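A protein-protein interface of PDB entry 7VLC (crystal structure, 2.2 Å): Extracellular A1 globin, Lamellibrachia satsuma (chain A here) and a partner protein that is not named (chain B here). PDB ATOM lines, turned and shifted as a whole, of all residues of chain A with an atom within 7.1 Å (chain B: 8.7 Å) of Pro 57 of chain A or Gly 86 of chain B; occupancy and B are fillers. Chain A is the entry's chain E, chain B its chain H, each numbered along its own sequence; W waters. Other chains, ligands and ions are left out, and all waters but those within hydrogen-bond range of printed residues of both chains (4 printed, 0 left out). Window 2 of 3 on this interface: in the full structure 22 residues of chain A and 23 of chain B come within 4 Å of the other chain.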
ATOM      1  N   VAL A  49     -15.210  11.535  15.047  1.00  0.00           N
ATOM      2  CA  VAL A  49     -13.815  11.175  14.838  1.00  0.00           C
ATOM      3  C   VAL A  49     -13.657   9.677  14.583  1.00  0.00           C
ATOM      4  O   VAL A  49     -12.602   9.111  14.845  1.00  0.00           O
ATOM      5  CB  VAL A  49     -12.937  11.643  16.016  1.00  0.00           C
ATOM      6  CG1 VAL A  49     -12.713  13.147  15.946  1.00  0.00           C
ATOM      7  CG2 VAL A  49     -13.574  11.257  17.353  1.00  0.00           C
ATOM      8  N   LYS A  50     -14.717   9.029  14.092  1.00  0.00           N
ATOM      9  CA  LYS A  50     -14.658   7.644  13.625  1.00  0.00           C
ATOM     10  C   LYS A  50     -14.246   6.688  14.749  1.00  0.00           C
ATOM     11  O   LYS A  50     -13.337   5.864  14.601  1.00  0.00           O
ATOM     12  CB  LYS A  50     -13.722   7.525  12.418  1.00  0.00           C
ATOM     13  CG  LYS A  50     -13.967   6.319  11.525  1.00  0.00           C
ATOM     14  CD  LYS A  50     -13.052   6.367  10.307  1.00  0.00           C
ATOM     15  CE  LYS A  50     -13.239   5.162   9.399  1.00  0.00           C
ATOM     16  NZ  LYS A  50     -12.306   5.217   8.231  1.00  0.00           N
ATOM     17  N   ASP A  53     -13.704   2.574  14.585  1.00  0.00           N
ATOM     18  CA  ASP A  53     -12.421   1.918  14.355  1.00  0.00           C
ATOM     19  C   ASP A  53     -11.355   2.745  15.058  1.00  0.00           C
ATOM     20  O   ASP A  53     -11.061   3.870  14.641  1.00  0.00           O
ATOM     21  CB  ASP A  53     -12.125   1.788  12.860  1.00  0.00           C
ATOM     22  CG  ASP A  53     -10.825   1.053  12.581  1.00  0.00           C
ATOM     23  OD1 ASP A  53     -10.312   0.367  13.491  1.00  0.00           O
ATOM     24  OD2 ASP A  53     -10.314   1.171  11.448  1.00  0.00           O
ATOM     25  N   MET A  54     -10.783   2.195  16.127  1.00  0.00           N
ATOM     26  CA  MET A  54      -9.853   2.965  16.941  1.00  0.00           C
ATOM     27  C   MET A  54      -8.471   3.085  16.313  1.00  0.00           C
ATOM     28  O   MET A  54      -7.691   3.945  16.734  1.00  0.00           O
ATOM     29  CB  MET A  54      -9.750   2.347  18.336  1.00  0.00           C
ATOM     30  CG  MET A  54     -11.089   2.298  19.061  1.00  0.00           C
ATOM     31  SD  MET A  54     -10.957   1.803  20.786  1.00  0.00           S
ATOM     32  CE  MET A  54     -10.018   3.177  21.444  1.00  0.00           C
ATOM     33  N   ARG A  55      -8.149   2.258  15.321  1.00  0.00           N
ATOM     34  CA  ARG A  55      -6.873   2.354  14.625  1.00  0.00           C
ATOM     35  C   ARG A  55      -6.983   3.163  13.338  1.00  0.00           C
ATOM     36  O   ARG A  55      -6.011   3.247  12.582  1.00  0.00           O
ATOM     37  CB  ARG A  55      -6.316   0.956  14.331  1.00  0.00           C
ATOM     38  CG  ARG A  55      -6.399  -0.028  15.505  1.00  0.00           C
ATOM     39  CD  ARG A  55      -5.963   0.600  16.833  1.00  0.00           C
ATOM     40  NE  ARG A  55      -4.515   0.605  17.025  1.00  0.00           N
ATOM     41  CZ  ARG A  55      -3.863  -0.221  17.840  1.00  0.00           C
ATOM     42  NH1 ARG A  55      -2.544  -0.142  17.952  1.00  0.00           N
ATOM     43  NH2 ARG A  55      -4.530  -1.124  18.547  1.00  0.00           N
ATOM     44  N   SER A  56      -8.144   3.761  13.078  1.00  0.00           N
ATOM     45  CA  SER A  56      -8.313   4.594  11.903  1.00  0.00           C
ATOM     46  C   SER A  56      -7.528   5.895  12.062  1.00  0.00           C
ATOM     47  O   SER A  56      -7.323   6.373  13.181  1.00  0.00           O
ATOM     48  CB  SER A  56      -9.790   4.905  11.677  1.00  0.00           C
ATOM     49  OG  SER A  56     -10.319   5.699  12.729  1.00  0.00           O
ATOM     50  N   PRO A  57      -7.074   6.489  10.955  1.00  0.00           N
ATOM     51  CA  PRO A  57      -6.340   7.763  11.062  1.00  0.00           C
ATOM     52  C   PRO A  57      -7.154   8.884  11.685  1.00  0.00           C
ATOM     53  O   PRO A  57      -6.572   9.772  12.320  1.00  0.00           O
ATOM     54  CB  PRO A  57      -5.962   8.077   9.603  1.00  0.00           C
ATOM     55  CG  PRO A  57      -6.894   7.260   8.769  1.00  0.00           C
ATOM     56  CD  PRO A  57      -7.149   6.011   9.562  1.00  0.00           C
ATOM     57  N   GLN A  58      -8.480   8.863  11.536  1.00  0.00           N
ATOM     58  CA  GLN A  58      -9.310   9.915  12.117  1.00  0.00           C
ATOM     59  C   GLN A  58      -9.331   9.833  13.641  1.00  0.00           C
ATOM     60  O   GLN A  58      -9.253  10.861  14.326  1.00  0.00           O
ATOM     61  CB  GLN A  58     -10.733   9.835  11.557  1.00  0.00           C
ATOM     62  CG  GLN A  58     -10.861  10.222  10.081  1.00  0.00           C
ATOM     63  CD  GLN A  58     -10.319   9.161   9.145  1.00  0.00           C
ATOM     64  OE1 GLN A  58     -10.269   7.981   9.490  1.00  0.00           O
ATOM     65  NE2 GLN A  58      -9.901   9.576   7.954  1.00  0.00           N
ATOM     66  N   PHE A  59      -9.440   8.626  14.196  1.00  0.00           N
ATOM     67  CA  PHE A  59      -9.495   8.520  15.648  1.00  0.00           C
ATOM     68  C   PHE A  59      -8.119   8.644  16.287  1.00  0.00           C
ATOM     69  O   PHE A  59      -8.005   9.196  17.388  1.00  0.00           O
ATOM     70  CB  PHE A  59     -10.149   7.209  16.077  1.00  0.00           C
ATOM     71  CG  PHE A  59     -10.495   7.179  17.534  1.00  0.00           C
ATOM     72  CD1 PHE A  59     -11.585   7.892  18.010  1.00  0.00           C
ATOM     73  CD2 PHE A  59      -9.707   6.477  18.435  1.00  0.00           C
ATOM     74  CE1 PHE A  59     -11.903   7.888  19.361  1.00  0.00           C
ATOM     75  CE2 PHE A  59     -10.018   6.466  19.788  1.00  0.00           C
ATOM     76  CZ  PHE A  59     -11.118   7.173  20.254  1.00  0.00           C
ATOM     77  N   LYS A  60      -7.073   8.142  15.624  1.00  0.00           N
ATOM     78  CA  LYS A  60      -5.722   8.340  16.138  1.00  0.00           C
ATOM     79  C   LYS A  60      -5.353   9.817  16.168  1.00  0.00           C
ATOM     80  O   LYS A  60      -4.587  10.250  17.035  1.00  0.00           O
ATOM     81  CB  LYS A  60      -4.722   7.543  15.301  1.00  0.00           C
ATOM     82  CG  LYS A  60      -4.876   6.034  15.459  1.00  0.00           C
ATOM     83  CD  LYS A  60      -3.645   5.277  14.994  1.00  0.00           C
ATOM     84  CE  LYS A  60      -3.477   5.335  13.487  1.00  0.00           C
ATOM     85  NZ  LYS A  60      -2.242   4.624  13.034  1.00  0.00           N
ATOM     86  N   ALA A  61      -5.898  10.605  15.244  1.00  0.00           N
ATOM     87  CA  ALA A  61      -5.678  12.045  15.280  1.00  0.00           C
ATOM     88  C   ALA A  61      -6.395  12.679  16.465  1.00  0.00           C
ATOM     89  O   ALA A  61      -5.879  13.620  17.082  1.00  0.00           O
ATOM     90  CB  ALA A  61      -6.135  12.675  13.963  1.00  0.00           C
ATOM     91  N   HIS A  62      -7.587  12.179  16.798  1.00  0.00           N
ATOM     92  CA  HIS A  62      -8.298  12.679  17.969  1.00  0.00           C
ATOM     93  C   HIS A  62      -7.547  12.327  19.246  1.00  0.00           C
ATOM     94  O   HIS A  62      -7.407  13.167  20.143  1.00  0.00           O
ATOM     95  CB  HIS A  62      -9.716  12.109  18.006  1.00  0.00           C
ATOM     96  CG  HIS A  62     -10.463  12.438  19.262  1.00  0.00           C
ATOM     97  ND1 HIS A  62     -10.965  13.696  19.520  1.00  0.00           N
ATOM     98  CD2 HIS A  62     -10.776  11.678  20.338  1.00  0.00           C
ATOM     99  CE1 HIS A  62     -11.562  13.695  20.698  1.00  0.00           C
ATOM    100  NE2 HIS A  62     -11.461  12.483  21.216  1.00  0.00           N
ATOM    101  N   ARG A  65      -4.803  14.726  19.670  1.00  0.00           N
ATOM    102  CA  ARG A  65      -5.270  16.042  20.105  1.00  0.00           C
ATOM    103  C   ARG A  65      -5.600  16.056  21.595  1.00  0.00           C
ATOM    104  O   ARG A  65      -5.313  17.041  22.288  1.00  0.00           O
ATOM    105  CB  ARG A  65      -6.489  16.477  19.283  1.00  0.00           C
ATOM    106  CG  ARG A  65      -6.150  16.963  17.880  1.00  0.00           C
ATOM    107  CD  ARG A  65      -7.339  17.627  17.187  1.00  0.00           C
ATOM    108  NE  ARG A  65      -8.406  16.681  16.871  1.00  0.00           N
ATOM    109  CZ  ARG A  65      -8.469  15.969  15.749  1.00  0.00           C
ATOM    110  NH1 ARG A  65      -7.521  16.085  14.830  1.00  0.00           N
ATOM    111  NH2 ARG A  65      -9.477  15.130  15.550  1.00  0.00           N
ATOM    112  N   PHE B   3       4.876  12.750   3.257  1.00  0.00           N
ATOM    113  CA  PHE B   3       5.439  14.022   3.695  1.00  0.00           C
ATOM    114  C   PHE B   3       6.950  14.066   3.461  1.00  0.00           C
ATOM    115  O   PHE B   3       7.425  14.752   2.555  1.00  0.00           O
ATOM    116  CB  PHE B   3       5.111  14.271   5.174  1.00  0.00           C
ATOM    117  CG  PHE B   3       3.680  14.673   5.415  1.00  0.00           C
ATOM    118  CD1 PHE B   3       2.679  13.718   5.476  1.00  0.00           C
ATOM    119  CD2 PHE B   3       3.335  16.009   5.566  1.00  0.00           C
ATOM    120  CE1 PHE B   3       1.363  14.082   5.686  1.00  0.00           C
ATOM    121  CE2 PHE B   3       2.018  16.381   5.776  1.00  0.00           C
ATOM    122  CZ  PHE B   3       1.031  15.416   5.836  1.00  0.00           C
ATOM    123  N   TYR B  81       4.165  12.796  14.332  1.00  0.00           N
ATOM    124  CA  TYR B  81       3.410  11.908  13.455  1.00  0.00           C
ATOM    125  C   TYR B  81       3.901  11.959  12.010  1.00  0.00           C
ATOM    126  O   TYR B  81       3.178  11.546  11.097  1.00  0.00           O
ATOM    127  CB  TYR B  81       1.917  12.235  13.526  1.00  0.00           C
ATOM    128  CG  TYR B  81       1.242  11.647  14.743  1.00  0.00           C
ATOM    129  CD1 TYR B  81       1.234  12.326  15.957  1.00  0.00           C
ATOM    130  CD2 TYR B  81       0.626  10.402  14.683  1.00  0.00           C
ATOM    131  CE1 TYR B  81       0.620  11.784  17.073  1.00  0.00           C
ATOM    132  CE2 TYR B  81       0.009   9.853  15.790  1.00  0.00           C
ATOM    133  CZ  TYR B  81       0.008  10.547  16.983  1.00  0.00           C
ATOM    134  OH  TYR B  81      -0.604  10.000  18.087  1.00  0.00           O
ATOM    135  N   LEU B  82       5.127  12.436  11.787  1.00  0.00           N
ATOM    136  CA  LEU B  82       5.660  12.520  10.429  1.00  0.00           C
ATOM    137  C   LEU B  82       5.793  11.149   9.773  1.00  0.00           C
ATOM    138  O   LEU B  82       5.724  11.046   8.543  1.00  0.00           O
ATOM    139  CB  LEU B  82       7.012  13.237  10.443  1.00  0.00           C
ATOM    140  CG  LEU B  82       6.974  14.766  10.492  1.00  0.00           C
ATOM    141  CD1 LEU B  82       8.348  15.341  10.815  1.00  0.00           C
ATOM    142  CD2 LEU B  82       6.464  15.312   9.168  1.00  0.00           C
ATOM    143  N   ASN B  83       5.990  10.090  10.560  1.00  0.00           N
ATOM    144  CA  ASN B  83       6.126   8.738  10.031  1.00  0.00           C
ATOM    145  C   ASN B  83       4.814   7.961  10.048  1.00  0.00           C
ATOM    146  O   ASN B  83       4.814   6.753   9.789  1.00  0.00           O
ATOM    147  CB  ASN B  83       7.203   7.968  10.802  1.00  0.00           C
ATOM    148  CG  ASN B  83       8.612   8.356  10.384  1.00  0.00           C
ATOM    149  OD1 ASN B  83       8.862   8.666   9.218  1.00  0.00           O
ATOM    150  ND2 ASN B  83       9.541   8.338  11.334  1.00  0.00           N
ATOM    151  N   ASP B  84       3.701   8.623  10.355  1.00  0.00           N
ATOM    152  CA  ASP B  84       2.359   8.052  10.266  1.00  0.00           C
ATOM    153  C   ASP B  84       1.578   8.954   9.315  1.00  0.00           C
ATOM    154  O   ASP B  84       0.828   9.832   9.750  1.00  0.00           O
ATOM    155  CB  ASP B  84       1.699   7.956  11.656  1.00  0.00           C
ATOM    156  CG  ASP B  84       0.434   7.117  11.649  1.00  0.00           C
ATOM    157  OD1 ASP B  84      -0.133   6.883  10.561  1.00  0.00           O
ATOM    158  OD2 ASP B  84      -0.001   6.697  12.744  1.00  0.00           O
ATOM    159  N   ALA B  85       1.766   8.727   8.012  1.00  0.00           N
ATOM    160  CA  ALA B  85       1.218   9.623   6.996  1.00  0.00           C
ATOM    161  C   ALA B  85      -0.302   9.699   7.060  1.00  0.00           C
ATOM    162  O   ALA B  85      -0.881  10.779   6.891  1.00  0.00           O
ATOM    163  CB  ALA B  85       1.670   9.173   5.605  1.00  0.00           C
ATOM    164  N   GLY B  86      -0.969   8.565   7.283  1.00  0.00           N
ATOM    165  CA  GLY B  86      -2.421   8.587   7.363  1.00  0.00           C
ATOM    166  C   GLY B  86      -2.923   9.434   8.518  1.00  0.00           C
ATOM    167  O   GLY B  86      -3.828  10.257   8.356  1.00  0.00           O
ATOM    168  N   THR B  87      -2.337   9.250   9.703  1.00  0.00           N
ATOM    169  CA  THR B  87      -2.751  10.052  10.850  1.00  0.00           C
ATOM    170  C   THR B  87      -2.349  11.507  10.673  1.00  0.00           C
ATOM    171  O   THR B  87      -3.127  12.413  10.997  1.00  0.00           O
ATOM    172  CB  THR B  87      -2.160   9.487  12.141  1.00  0.00           C
ATOM    173  OG1 THR B  87      -2.586   8.134  12.302  1.00  0.00           O
ATOM    174  CG2 THR B  87      -2.637  10.294  13.341  1.00  0.00           C
ATOM    175  N   LEU B  88      -1.142  11.752  10.157  1.00  0.00           N
ATOM    176  CA  LEU B  88      -0.701  13.126   9.950  1.00  0.00           C
ATOM    177  C   LEU B  88      -1.578  13.849   8.933  1.00  0.00           C
ATOM    178  O   LEU B  88      -1.807  15.057   9.061  1.00  0.00           O
ATOM    179  CB  LEU B  88       0.762  13.145   9.509  1.00  0.00           C
ATOM    180  CG  LEU B  88       1.389  14.536   9.375  1.00  0.00           C
ATOM    181  CD1 LEU B  88       1.193  15.326  10.659  1.00  0.00           C
ATOM    182  CD2 LEU B  88       2.865  14.434   9.027  1.00  0.00           C
ATOM    183  N   THR B  89      -2.087  13.131   7.928  1.00  0.00           N
ATOM    184  CA  THR B  89      -2.990  13.745   6.957  1.00  0.00           C
ATOM    185  C   THR B  89      -4.286  14.186   7.625  1.00  0.00           C
ATOM    186  O   THR B  89      -4.815  15.264   7.330  1.00  0.00           O
ATOM    187  CB  THR B  89      -3.271  12.767   5.815  1.00  0.00           C
ATOM    188  OG1 THR B  89      -2.055  12.525   5.090  1.00  0.00           O
ATOM    189  CG2 THR B  89      -4.332  13.320   4.859  1.00  0.00           C
ATOM    190  N   SER B  90      -4.798  13.371   8.547  1.00  0.00           N
ATOM    191  CA  SER B  90      -5.994  13.740   9.294  1.00  0.00           C
ATOM    192  C   SER B  90      -5.704  14.841  10.307  1.00  0.00           C
ATOM    193  O   SER B  90      -6.572  15.677  10.584  1.00  0.00           O
ATOM    194  CB  SER B  90      -6.561  12.501   9.987  1.00  0.00           C
ATOM    195  OG  SER B  90      -7.755  12.803  10.673  1.00  0.00           O
ATOM    196  N   LEU B  91      -4.492  14.860  10.866  1.00  0.00           N
ATOM    197  CA  LEU B  91      -4.126  15.891  11.830  1.00  0.00           C
ATOM    198  C   LEU B  91      -4.001  17.252  11.157  1.00  0.00           C
ATOM    199  O   LEU B  91      -4.495  18.260  11.675  1.00  0.00           O
ATOM    200  CB  LEU B  91      -2.815  15.519  12.522  1.00  0.00           C
ATOM    201  CG  LEU B  91      -2.894  14.570  13.716  1.00  0.00           C
ATOM    202  CD1 LEU B  91      -1.494  14.169  14.157  1.00  0.00           C
ATOM    203  CD2 LEU B  91      -3.654  15.227  14.862  1.00  0.00           C
ATOM    204  N   THR B  92      -3.333  17.301  10.003  1.00  0.00           N
ATOM    205  CA  THR B  92      -3.152  18.571   9.311  1.00  0.00           C
ATOM    206  C   THR B  92      -4.458  19.070   8.706  1.00  0.00           C
ATOM    207  O   THR B  92      -4.690  20.284   8.659  1.00  0.00           O
ATOM    208  CB  THR B  92      -2.086  18.429   8.227  1.00  0.00           C
ATOM    209  OG1 THR B  92      -2.433  17.353   7.350  1.00  0.00           O
ATOM    210  CG2 THR B  92      -0.720  18.148   8.850  1.00  0.00           C
ATOM    211  N   ALA B  93      -5.316  18.157   8.240  1.00  0.00           N
ATOM    212  CA  ALA B  93      -6.607  18.566   7.693  1.00  0.00           C
ATOM    213  C   ALA B  93      -7.470  19.216   8.765  1.00  0.00           C
ATOM    214  O   ALA B  93      -8.166  20.202   8.498  1.00  0.00           O
ATOM    215  CB  ALA B  93      -7.326  17.364   7.077  1.00  0.00           C
HETATM  216  O   HOH W   1      -8.600  15.120  12.220  1.00  0.00           O
HETATM  217  O   HOH W   2      -9.629  12.884   8.257  1.00  0.00           O
HETATM  218  O   HOH W   3      -5.283  18.236  14.409  1.00  0.00           O
HETATM  219  O   HOH W   4      -2.728   8.723  18.205  1.00  0.00           O
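Among the printed residues, merely in contact across the chains: Lys 60 of chain A with Thr 87 of chain B, Pro 57 of chain A with Gly 86 of chain B, Ala 61 of chain A with Leu 91 of chain B, Gln 58 of chain A with Ser 90 of chain B, Pro 57 of chain A with Ser 90 of chain B, Ala 61 of chain A with Ser 90 of chain B, Ala 61 of chain A with Thr 87 of chain B, Pro 57 of chain A with Thr 87 of chain B and Arg 65 of chain A with Leu 91 of chain B.
OD2 of Asp 84 of chain B is in hydrogen-bond range of OG1 of Thr 87 of chain B (3.0 Å).
Water W4 lies within hydrogen-bond range of the side-chain hydroxyl (OH) of Tyr 81 of chain B and the backbone carbonyl oxygen (O) of Lys 60 of chain A.
Water W1 lies within hydrogen-bond range of O of Ser 90 of chain B (2.7 Å) and NH1 of Arg 65 of chain A (3.0 Å).
Water W3 lies within hydrogen-bond range of O of Leu 91 of chain B and NH1 of Arg 65 of chain A.
Water W2 bridges OG of Ser 90 of chain B (3.1 Å) and NE2 of Gln 58 of chain A (3.3 Å).
Lys 50 of chain A touches none of the printed residues of chain B.
No residue of chain B comes within 4 Å of Ser 56 of chain A.
Pro 57 of chain A touches three residues of chain B.
Gln 58 of chain A touches just one residue of chain B: Ser 90 (3.6 Å).
Of the printed residues of chain B, Arg 65 of chain A touches Leu 91.
Of chain A, only Pro 57 (3.3 Å) comes within 4 Å of Gly 86 of chain B.
Of the printed residues of chain A, Thr 87 of chain B touches Pro 57 (3.8 Å), Lys 60 (3.2 Å) and Ala 61 (3.8 Å).
Printed residues of chain A within 4 Å of Leu 91 of chain B: Ala 61 (3.5 Å) and Arg 65 (3.96 Å).
Thr 92 of chain B touches none of the printed residues of chain A.
The nearest residue of chain B that does not touch Pro 57 of chain A is Leu 91 of chain B (5.7 Å).
Hydrophobic or aromatic side chains of chain A that line the printed part of chain B: Pro 57 and Ala 61.
Along chain A the printed residues that touch a printed residue of chain B span positions 57 to 65.
Of the 14 printed residues of chain B, 5 touch a printed residue of chain A.
Along chain B the printed residues that touch a printed residue of chain A span positions 84 to 91.
Among the printed residues, 10 pairs touch across the chains.
Among the printed residues, Asp or Glu carboxylates within 4 Å of a Lys or Arg side-chain nitrogen of the other chain: Lys 60 of chain A with Asp 84 of chain B.
The side-chain amino group (NZ) of Lys 60 of chain A is in salt-bridge range of the side-chain carboxylate (OD2) of Asp 84 of chain B, at 3.1 Å.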
